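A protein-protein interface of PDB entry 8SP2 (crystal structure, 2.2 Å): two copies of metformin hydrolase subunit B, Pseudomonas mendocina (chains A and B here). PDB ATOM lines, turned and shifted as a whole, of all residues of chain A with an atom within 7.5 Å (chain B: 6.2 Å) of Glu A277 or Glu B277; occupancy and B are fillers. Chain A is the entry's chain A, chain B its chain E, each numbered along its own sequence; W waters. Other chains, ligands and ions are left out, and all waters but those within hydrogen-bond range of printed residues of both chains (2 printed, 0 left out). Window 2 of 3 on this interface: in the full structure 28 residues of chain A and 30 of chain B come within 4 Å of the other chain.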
ATOM      1  N   MET A 225      21.076  33.044  -2.820  1.00  0.00           N
ATOM      2  CA  MET A 225      20.747  31.630  -2.859  1.00  0.00           C
ATOM      3  C   MET A 225      20.947  31.114  -4.282  1.00  0.00           C
ATOM      4  O   MET A 225      21.375  29.969  -4.460  1.00  0.00           O
ATOM      5  CB  MET A 225      19.312  31.374  -2.382  1.00  0.00           C
ATOM      6  CG  MET A 225      19.004  29.928  -2.025  1.00  0.00           C
ATOM      7  SD  MET A 225      20.022  29.316  -0.655  1.00  0.00           S
ATOM      8  CE  MET A 225      19.228  30.018   0.776  1.00  0.00           C
ATOM      9  N   PHE A 229      23.093  27.902  -5.250  1.00  0.00           N
ATOM     10  CA  PHE A 229      22.617  26.763  -6.048  1.00  0.00           C
ATOM     11  C   PHE A 229      23.472  26.566  -7.303  1.00  0.00           C
ATOM     12  O   PHE A 229      23.810  25.433  -7.631  1.00  0.00           O
ATOM     13  CB  PHE A 229      21.152  26.936  -6.459  1.00  0.00           C
ATOM     14  CG  PHE A 229      20.168  26.773  -5.325  1.00  0.00           C
ATOM     15  CD1 PHE A 229      20.475  25.999  -4.216  1.00  0.00           C
ATOM     16  CD2 PHE A 229      18.936  27.414  -5.344  1.00  0.00           C
ATOM     17  CE1 PHE A 229      19.574  25.850  -3.174  1.00  0.00           C
ATOM     18  CE2 PHE A 229      18.044  27.270  -4.286  1.00  0.00           C
ATOM     19  CZ  PHE A 229      18.365  26.496  -3.206  1.00  0.00           C
ATOM     20  N   ILE A 233      26.536  25.033  -3.877  1.00  0.00           N
ATOM     21  CA  ILE A 233      26.489  25.502  -2.502  1.00  0.00           C
ATOM     22  C   ILE A 233      27.879  25.448  -1.887  1.00  0.00           C
ATOM     23  O   ILE A 233      28.446  26.492  -1.613  1.00  0.00           O
ATOM     24  CB  ILE A 233      25.434  24.761  -1.644  1.00  0.00           C
ATOM     25  CG1 ILE A 233      24.019  24.812  -2.243  1.00  0.00           C
ATOM     26  CG2 ILE A 233      25.432  25.300  -0.225  1.00  0.00           C
ATOM     27  CD1 ILE A 233      23.014  23.906  -1.541  1.00  0.00           C
ATOM     28  N   TYR A 234      28.414  24.252  -1.609  1.00  0.00           N
ATOM     29  CA  TYR A 234      29.511  24.137  -0.651  1.00  0.00           C
ATOM     30  C   TYR A 234      30.788  24.818  -1.158  1.00  0.00           C
ATOM     31  O   TYR A 234      31.459  25.497  -0.373  1.00  0.00           O
ATOM     32  CB  TYR A 234      29.760  22.674  -0.282  1.00  0.00           C
ATOM     33  CG  TYR A 234      28.505  21.949   0.128  1.00  0.00           C
ATOM     34  CD1 TYR A 234      27.744  22.412   1.190  1.00  0.00           C
ATOM     35  CD2 TYR A 234      28.042  20.850  -0.588  1.00  0.00           C
ATOM     36  CE1 TYR A 234      26.560  21.790   1.549  1.00  0.00           C
ATOM     37  CE2 TYR A 234      26.868  20.211  -0.229  1.00  0.00           C
ATOM     38  CZ  TYR A 234      26.124  20.686   0.839  1.00  0.00           C
ATOM     39  OH  TYR A 234      24.971  20.054   1.213  1.00  0.00           O
ATOM     40  N   VAL A 259      16.856  31.627   6.188  1.00  0.00           N
ATOM     41  CA  VAL A 259      17.788  31.076   5.209  1.00  0.00           C
ATOM     42  C   VAL A 259      17.277  29.722   4.675  1.00  0.00           C
ATOM     43  O   VAL A 259      17.631  29.337   3.550  1.00  0.00           O
ATOM     44  CB  VAL A 259      19.207  30.900   5.779  1.00  0.00           C
ATOM     45  CG1 VAL A 259      19.267  29.800   6.828  1.00  0.00           C
ATOM     46  CG2 VAL A 259      20.234  30.648   4.681  1.00  0.00           C
ATOM     47  N   MET A 260      16.566  28.966   5.524  1.00  0.00           N
ATOM     48  CA  MET A 260      16.188  27.592   5.209  1.00  0.00           C
ATOM     49  C   MET A 260      14.965  27.645   4.309  1.00  0.00           C
ATOM     50  O   MET A 260      14.222  28.616   4.339  1.00  0.00           O
ATOM     51  CB  MET A 260      15.813  26.781   6.458  1.00  0.00           C
ATOM     52  CG  MET A 260      16.858  26.743   7.566  1.00  0.00           C
ATOM     53  SD  MET A 260      18.472  26.071   7.058  1.00  0.00           S
ATOM     54  CE  MET A 260      17.984  24.412   6.551  1.00  0.00           C
ATOM     55  N   ASP A 261      14.750  26.574   3.552  1.00  0.00           N
ATOM     56  CA  ASP A 261      13.521  26.366   2.816  1.00  0.00           C
ATOM     57  C   ASP A 261      12.357  26.452   3.796  1.00  0.00           C
ATOM     58  O   ASP A 261      12.463  25.972   4.922  1.00  0.00           O
ATOM     59  CB  ASP A 261      13.573  24.995   2.136  1.00  0.00           C
ATOM     60  CG  ASP A 261      12.580  24.831   1.006  1.00  0.00           C
ATOM     61  OD1 ASP A 261      12.743  25.541   0.019  1.00  0.00           O
ATOM     62  OD2 ASP A 261      11.685  23.995   1.117  1.00  0.00           O
ATOM     63  N   SER A 263       9.795  24.711   3.973  1.00  0.00           N
ATOM     64  CA  SER A 263       9.410  23.368   4.393  1.00  0.00           C
ATOM     65  C   SER A 263      10.081  23.003   5.712  1.00  0.00           C
ATOM     66  O   SER A 263       9.420  22.417   6.552  1.00  0.00           O
ATOM     67  CB  SER A 263       9.702  22.333   3.336  1.00  0.00           C
ATOM     68  OG  SER A 263      11.086  22.248   2.984  1.00  0.00           O
ATOM     69  N   THR A 264      11.353  23.389   5.904  1.00  0.00           N
ATOM     70  CA  THR A 264      12.031  23.065   7.147  1.00  0.00           C
ATOM     71  C   THR A 264      12.012  24.224   8.138  1.00  0.00           C
ATOM     72  O   THR A 264      12.601  24.111   9.203  1.00  0.00           O
ATOM     73  CB  THR A 264      13.547  22.857   7.020  1.00  0.00           C
ATOM     74  OG1 THR A 264      13.998  22.720   5.674  1.00  0.00           O
ATOM     75  CG2 THR A 264      14.011  21.699   7.870  1.00  0.00           C
ATOM     76  N   GLY A 274      12.320  28.004  -1.263  1.00  0.00           N
ATOM     77  CA  GLY A 274      13.475  27.837  -2.148  1.00  0.00           C
ATOM     78  C   GLY A 274      14.839  28.126  -1.487  1.00  0.00           C
ATOM     79  O   GLY A 274      15.740  28.690  -2.112  1.00  0.00           O
ATOM     80  N   GLY A 275      15.020  27.654  -0.250  1.00  0.00           N
ATOM     81  CA  GLY A 275      16.240  27.896   0.519  1.00  0.00           C
ATOM     82  C   GLY A 275      16.967  26.588   0.805  1.00  0.00           C
ATOM     83  O   GLY A 275      16.682  25.545   0.174  1.00  0.00           O
ATOM     84  N   LEU A 276      17.880  26.659   1.777  1.00  0.00           N
ATOM     85  CA  LEU A 276      18.680  25.514   2.169  1.00  0.00           C
ATOM     86  C   LEU A 276      17.789  24.427   2.751  1.00  0.00           C
ATOM     87  O   LEU A 276      16.791  24.735   3.410  1.00  0.00           O
ATOM     88  CB  LEU A 276      19.691  25.958   3.232  1.00  0.00           C
ATOM     89  CG  LEU A 276      20.851  26.799   2.703  1.00  0.00           C
ATOM     90  CD1 LEU A 276      21.739  27.275   3.848  1.00  0.00           C
ATOM     91  CD2 LEU A 276      21.665  25.994   1.694  1.00  0.00           C
ATOM     92  N   GLU A 277      18.171  23.159   2.524  1.00  0.00           N
ATOM     93  CA  GLU A 277      17.516  22.041   3.186  1.00  0.00           C
ATOM     94  C   GLU A 277      18.392  21.624   4.367  1.00  0.00           C
ATOM     95  O   GLU A 277      19.550  22.019   4.441  1.00  0.00           O
ATOM     96  CB  GLU A 277      17.178  20.966   2.148  1.00  0.00           C
ATOM     97  CG  GLU A 277      15.821  21.247   1.497  1.00  0.00           C
ATOM     98  CD  GLU A 277      15.552  20.777   0.081  1.00  0.00           C
ATOM     99  OE1 GLU A 277      14.637  21.364  -0.575  1.00  0.00           O
ATOM    100  OE2 GLU A 277      16.232  19.832  -0.357  1.00  0.00           O
ATOM    101  N   SER A 278      17.810  20.869   5.303  1.00  0.00           N
ATOM    102  CA  SER A 278      18.406  20.567   6.600  1.00  0.00           C
ATOM    103  C   SER A 278      19.795  19.948   6.476  1.00  0.00           C
ATOM    104  O   SER A 278      20.703  20.371   7.172  1.00  0.00           O
ATOM    105  CB  SER A 278      17.502  19.645   7.407  1.00  0.00           C
ATOM    106  OG  SER A 278      17.328  18.384   6.748  1.00  0.00           O
ATOM    107  N   ARG A 279      19.939  18.897   5.657  1.00  0.00           N
ATOM    108  CA  ARG A 279      21.213  18.217   5.457  1.00  0.00           C
ATOM    109  C   ARG A 279      22.270  19.170   4.907  1.00  0.00           C
ATOM    110  O   ARG A 279      23.442  18.970   5.179  1.00  0.00           O
ATOM    111  CB  ARG A 279      21.077  17.013   4.519  1.00  0.00           C
ATOM    112  CG  ARG A 279      20.770  17.345   3.066  1.00  0.00           C
ATOM    113  CD  ARG A 279      20.603  16.100   2.178  1.00  0.00           C
ATOM    114  NE  ARG A 279      19.414  15.296   2.455  1.00  0.00           N
ATOM    115  CZ  ARG A 279      18.911  14.373   1.624  1.00  0.00           C
ATOM    116  NH1 ARG A 279      19.562  14.029   0.530  1.00  0.00           N
ATOM    117  NH2 ARG A 279      17.767  13.761   1.897  1.00  0.00           N
ATOM    118  N   GLU A 280      21.865  20.188   4.128  1.00  0.00           N
ATOM    119  CA  GLU A 280      22.795  21.146   3.555  1.00  0.00           C
ATOM    120  C   GLU A 280      23.351  22.057   4.646  1.00  0.00           C
ATOM    121  O   GLU A 280      24.558  22.316   4.685  1.00  0.00           O
ATOM    122  CB  GLU A 280      22.133  21.950   2.438  1.00  0.00           C
ATOM    123  CG  GLU A 280      21.860  21.123   1.187  1.00  0.00           C
ATOM    124  CD  GLU A 280      20.835  21.711   0.232  1.00  0.00           C
ATOM    125  OE1 GLU A 280      20.102  22.643   0.610  1.00  0.00           O
ATOM    126  OE2 GLU A 280      20.802  21.247  -0.896  1.00  0.00           O
ATOM    127  N   MET A 281      22.479  22.517   5.542  1.00  0.00           N
ATOM    128  CA  MET A 281      22.926  23.368   6.642  1.00  0.00           C
ATOM    129  C   MET A 281      23.822  22.565   7.595  1.00  0.00           C
ATOM    130  O   MET A 281      24.745  23.115   8.177  1.00  0.00           O
ATOM    131  CB  MET A 281      21.737  23.966   7.408  1.00  0.00           C
ATOM    132  CG  MET A 281      22.162  24.894   8.568  1.00  0.00           C
ATOM    133  SD  MET A 281      23.298  26.228   8.030  1.00  0.00           S
ATOM    134  CE  MET A 281      22.132  27.578   7.902  1.00  0.00           C
ATOM    135  N   MET A 282      23.561  21.261   7.750  1.00  0.00           N
ATOM    136  CA  MET A 282      24.376  20.380   8.581  1.00  0.00           C
ATOM    137  C   MET A 282      25.798  20.292   8.042  1.00  0.00           C
ATOM    138  O   MET A 282      26.757  20.396   8.798  1.00  0.00           O
ATOM    139  CB  MET A 282      23.822  18.957   8.617  1.00  0.00           C
ATOM    140  CG  MET A 282      23.398  18.579   9.971  1.00  0.00           C
ATOM    141  SD  MET A 282      21.914  19.476  10.420  1.00  0.00           S
ATOM    142  CE  MET A 282      20.758  18.202   9.914  1.00  0.00           C
ATOM    143  N   ARG A 283      25.908  20.098   6.726  1.00  0.00           N
ATOM    144  CA  ARG A 283      27.202  20.045   6.079  1.00  0.00           C
ATOM    145  C   ARG A 283      27.915  21.380   6.294  1.00  0.00           C
ATOM    146  O   ARG A 283      29.086  21.415   6.676  1.00  0.00           O
ATOM    147  CB  ARG A 283      27.028  19.655   4.609  1.00  0.00           C
ATOM    148  CG  ARG A 283      28.332  19.658   3.825  1.00  0.00           C
ATOM    149  CD  ARG A 283      29.036  18.315   3.769  1.00  0.00           C
ATOM    150  NE  ARG A 283      28.737  17.645   2.508  1.00  0.00           N
ATOM    151  CZ  ARG A 283      29.280  17.954   1.330  1.00  0.00           C
ATOM    152  NH1 ARG A 283      30.317  18.775   1.248  1.00  0.00           N
ATOM    153  NH2 ARG A 283      28.799  17.402   0.229  1.00  0.00           N
ATOM    154  N   ILE A 284      27.188  22.481   6.093  1.00  0.00           N
ATOM    155  CA  ILE A 284      27.757  23.809   6.262  1.00  0.00           C
ATOM    156  C   ILE A 284      28.295  24.020   7.680  1.00  0.00           C
ATOM    157  O   ILE A 284      29.338  24.637   7.866  1.00  0.00           O
ATOM    158  CB  ILE A 284      26.715  24.866   5.870  1.00  0.00           C
ATOM    159  CG1 ILE A 284      26.537  24.883   4.351  1.00  0.00           C
ATOM    160  CG2 ILE A 284      27.100  26.230   6.405  1.00  0.00           C
ATOM    161  CD1 ILE A 284      25.255  25.449   3.886  1.00  0.00           C
ATOM    162  N   LEU A 315      14.716  22.448  14.055  1.00  0.00           N
ATOM    163  CA  LEU A 315      15.849  22.516  13.158  1.00  0.00           C
ATOM    164  C   LEU A 315      16.894  23.455  13.731  1.00  0.00           C
ATOM    165  O   LEU A 315      18.088  23.152  13.657  1.00  0.00           O
ATOM    166  CB  LEU A 315      15.491  23.010  11.764  1.00  0.00           C
ATOM    167  CG  LEU A 315      16.774  23.105  10.932  1.00  0.00           C
ATOM    168  CD1 LEU A 315      16.877  21.994   9.910  1.00  0.00           C
ATOM    169  CD2 LEU A 315      16.920  24.471  10.331  1.00  0.00           C
ATOM    170  N   MET B 260      12.717   9.657   7.864  1.00  0.00           N
ATOM    171  CA  MET B 260      12.474  10.731   6.908  1.00  0.00           C
ATOM    172  C   MET B 260      12.829  12.057   7.564  1.00  0.00           C
ATOM    173  O   MET B 260      12.859  12.170   8.781  1.00  0.00           O
ATOM    174  CB  MET B 260      10.998  10.811   6.507  1.00  0.00           C
ATOM    175  CG  MET B 260      10.417   9.505   6.040  1.00  0.00           C
ATOM    176  SD  MET B 260      11.265   8.782   4.636  1.00  0.00           S
ATOM    177  CE  MET B 260      11.017  10.047   3.387  1.00  0.00           C
ATOM    178  N   ASP B 261      13.115  13.049   6.732  1.00  0.00           N
ATOM    179  CA  ASP B 261      13.305  14.407   7.203  1.00  0.00           C
ATOM    180  C   ASP B 261      12.011  14.894   7.867  1.00  0.00           C
ATOM    181  O   ASP B 261      10.921  14.543   7.433  1.00  0.00           O
ATOM    182  CB  ASP B 261      13.749  15.256   6.013  1.00  0.00           C
ATOM    183  CG  ASP B 261      14.324  16.607   6.394  1.00  0.00           C
ATOM    184  OD1 ASP B 261      15.309  16.626   7.150  1.00  0.00           O
ATOM    185  OD2 ASP B 261      13.748  17.623   5.942  1.00  0.00           O
ATOM    186  N   THR B 264       9.039  16.192   5.953  1.00  0.00           N
ATOM    187  CA  THR B 264       8.347  15.141   5.222  1.00  0.00           C
ATOM    188  C   THR B 264       7.452  14.303   6.131  1.00  0.00           C
ATOM    189  O   THR B 264       6.554  13.621   5.641  1.00  0.00           O
ATOM    190  CB  THR B 264       9.354  14.159   4.609  1.00  0.00           C
ATOM    191  OG1 THR B 264      10.430  14.901   4.043  1.00  0.00           O
ATOM    192  CG2 THR B 264       8.758  13.290   3.530  1.00  0.00           C
ATOM    193  N   GLY B 275      16.929  13.854   7.532  1.00  0.00           N
ATOM    194  CA  GLY B 275      16.598  12.516   7.056  1.00  0.00           C
ATOM    195  C   GLY B 275      16.319  12.442   5.552  1.00  0.00           C
ATOM    196  O   GLY B 275      16.607  13.355   4.790  1.00  0.00           O
ATOM    197  N   LEU B 276      15.748  11.312   5.135  1.00  0.00           N
ATOM    198  CA  LEU B 276      15.451  11.035   3.742  1.00  0.00           C
ATOM    199  C   LEU B 276      14.356  11.967   3.234  1.00  0.00           C
ATOM    200  O   LEU B 276      13.456  12.344   3.982  1.00  0.00           O
ATOM    201  CB  LEU B 276      14.989   9.578   3.632  1.00  0.00           C
ATOM    202  CG  LEU B 276      16.079   8.514   3.738  1.00  0.00           C
ATOM    203  CD1 LEU B 276      15.479   7.125   3.667  1.00  0.00           C
ATOM    204  CD2 LEU B 276      17.108   8.690   2.637  1.00  0.00           C
ATOM    205  N   GLU B 277      14.456  12.322   1.951  1.00  0.00           N
ATOM    206  CA  GLU B 277      13.370  12.951   1.222  1.00  0.00           C
ATOM    207  C   GLU B 277      12.442  11.869   0.681  1.00  0.00           C
ATOM    208  O   GLU B 277      12.864  10.731   0.467  1.00  0.00           O
ATOM    209  CB  GLU B 277      13.870  13.739   0.012  1.00  0.00           C
ATOM    210  CG  GLU B 277      14.869  14.838   0.330  1.00  0.00           C
ATOM    211  CD  GLU B 277      15.520  15.423  -0.918  1.00  0.00           C
ATOM    212  OE1 GLU B 277      15.245  14.892  -2.021  1.00  0.00           O
ATOM    213  OE2 GLU B 277      16.280  16.420  -0.798  1.00  0.00           O
ATOM    214  N   SER B 278      11.196  12.264   0.409  1.00  0.00           N
ATOM    215  CA  SER B 278      10.168  11.342  -0.046  1.00  0.00           C
ATOM    216  C   SER B 278      10.604  10.636  -1.331  1.00  0.00           C
ATOM    217  O   SER B 278      10.355   9.450  -1.504  1.00  0.00           O
ATOM    218  CB  SER B 278       8.842  12.059  -0.239  1.00  0.00           C
ATOM    219  OG  SER B 278       8.978  13.145  -1.156  1.00  0.00           O
ATOM    220  N   ARG B 279      11.214  11.373  -2.259  1.00  0.00           N
ATOM    221  CA  ARG B 279      11.584  10.777  -3.531  1.00  0.00           C
ATOM    222  C   ARG B 279      12.723   9.770  -3.395  1.00  0.00           C
ATOM    223  O   ARG B 279      12.823   8.842  -4.201  1.00  0.00           O
ATOM    224  CB  ARG B 279      11.968  11.842  -4.539  1.00  0.00           C
ATOM    225  CG  ARG B 279      13.128  12.753  -4.168  1.00  0.00           C
ATOM    226  CD  ARG B 279      12.837  13.736  -5.264  1.00  0.00           C
ATOM    227  NE  ARG B 279      13.549  14.966  -5.376  1.00  0.00           N
ATOM    228  CZ  ARG B 279      13.142  15.966  -6.136  1.00  0.00           C
ATOM    229  NH1 ARG B 279      11.874  16.322  -6.171  1.00  0.00           N
ATOM    230  NH2 ARG B 279      14.044  16.717  -6.721  1.00  0.00           N
ATOM    231  N   GLU B 280      13.546   9.946  -2.359  1.00  0.00           N
ATOM    232  CA  GLU B 280      14.605   8.996  -2.039  1.00  0.00           C
ATOM    233  C   GLU B 280      13.992   7.688  -1.534  1.00  0.00           C
ATOM    234  O   GLU B 280      14.431   6.603  -1.913  1.00  0.00           O
ATOM    235  CB  GLU B 280      15.575   9.622  -1.031  1.00  0.00           C
ATOM    236  CG  GLU B 280      16.456  10.722  -1.626  1.00  0.00           C
ATOM    237  CD  GLU B 280      17.157  11.614  -0.606  1.00  0.00           C
ATOM    238  OE1 GLU B 280      16.773  11.538   0.575  1.00  0.00           O
ATOM    239  OE2 GLU B 280      18.080  12.394  -0.995  1.00  0.00           O
ATOM    240  N   MET B 281      12.983   7.790  -0.662  1.00  0.00           N
ATOM    241  CA  MET B 281      12.341   6.606  -0.122  1.00  0.00           C
ATOM    242  C   MET B 281      11.596   5.881  -1.237  1.00  0.00           C
ATOM    243  O   MET B 281      11.512   4.659  -1.207  1.00  0.00           O
ATOM    244  CB  MET B 281      11.385   6.943   1.028  1.00  0.00           C
ATOM    245  CG  MET B 281      10.701   5.742   1.654  1.00  0.00           C
ATOM    246  SD  MET B 281      11.851   4.442   2.176  1.00  0.00           S
ATOM    247  CE  MET B 281      12.294   5.003   3.820  1.00  0.00           C
ATOM    248  N   MET B 282      11.058   6.612  -2.222  1.00  0.00           N
ATOM    249  CA  MET B 282      10.308   5.956  -3.280  1.00  0.00           C
ATOM    250  C   MET B 282      11.273   5.157  -4.156  1.00  0.00           C
ATOM    251  O   MET B 282      10.943   4.065  -4.601  1.00  0.00           O
ATOM    252  CB  MET B 282       9.511   6.936  -4.148  1.00  0.00           C
ATOM    253  CG  MET B 282       8.441   7.731  -3.401  1.00  0.00           C
ATOM    254  SD  MET B 282       7.583   6.792  -2.135  1.00  0.00           S
ATOM    255  CE  MET B 282       6.348   7.969  -1.588  1.00  0.00           C
HETATM  256  O   HOH W   1      17.669  15.645   5.040  1.00  0.00           O
HETATM  257  O   HOH W   2      14.999  19.941   4.979  1.00  0.00           O
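The side-chain carboxylate of Glu A280 sits at hydrogen-bond distance from the backbone NH of Glu A277, at 2.8 Å.
OG1 of Thr B264 lies close to O of Asp B261, at 3.4 Å.
The side-chain carboxylate (OD1) of Asp B261 lies within hydrogen-bond range of the backbone NH (N) of Gly B275, at 3.2 Å.
N of Asp B261 is in hydrogen-bond range of O of Leu B276, 2.9 Å away.
The guanidinium group (NE) of Arg B279 is in salt-bridge range of the side-chain carboxylate (OE1) of Glu B277 (3.8 Å).
The backbone NH (N) of Glu B277 sits at hydrogen-bond distance from the side-chain carboxylate (OE1) of Glu B280 (2.8 Å).
Arg A279 touches Glu B277.
Ser A278 touches Asp B261, but with the chains exchanged Asp A261 does not touch Ser B278 (11.4 Å).
Arg A279 touches Gly B275, but with the chains exchanged Gly A275 does not touch Arg B279 (11.5 Å).
Arg A279 touches Glu B277, but with the chains exchanged Glu A277 does not touch Arg B279 (7.4 Å).
Arg A279 touches Glu B280, but with the chains exchanged Glu A280 does not touch Arg B279 (10.0 Å).
11 positions are printed for both chains.
Of the 5 pairs that touch across the chains among the printed residues, 1 has its exchanged pair printed and touching as well.
Printed residues of chain B within 4 Å of Glu A277: Glu B277 (3.4 Å).
Of the printed residues of chain B, Ser A278 touches Asp B261.
Glu B277 touches two residues of chain A.
Printed residues of chain A within 4 Å of Glu B280: Arg A279.
The nearest residue of chain B that does not touch Glu A277 is Asp B261 (6.1 Å).
The nearest printed residue of chain B that does not touch Ser A278 is Gly B275 (4.6 Å).
Water W1 lies within hydrogen-bond range of O of Gly B275 (2.5 Å), NE of Arg A279 (3.1 Å), OG of Ser A278 (3.2 Å) and OD1 of Asp B261 (3.3 Å).
Water W2 lies within hydrogen-bond range of OD2 of Asp B261, N of Ser A278 and OG1 of Thr A264.
OG of Ser A278 lies within hydrogen-bond range of OD1 of Asp B261 (2.7 Å).
The guanidinium group (NH2) of Arg A279 sits at hydrogen-bond distance from the backbone carbonyl oxygen (O) of Gly B275, 3.1 Å away.
The side-chain carboxylate (OE2) of Glu B280 is in salt-bridge range of the guanidinium group (NH1) of Arg A279 (2.7 Å).
OE2 of Glu B277 sits close to OE2 of Glu A277 (3.4 Å).
Of the 21 printed residues of chain A, 3 touch a printed residue of chain B.
Among the printed residues, Asp or Glu carboxylates within 4 Å of a Lys or Arg side-chain nitrogen of the other chain: Arg A279 with Glu B280 (2.7 Å).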
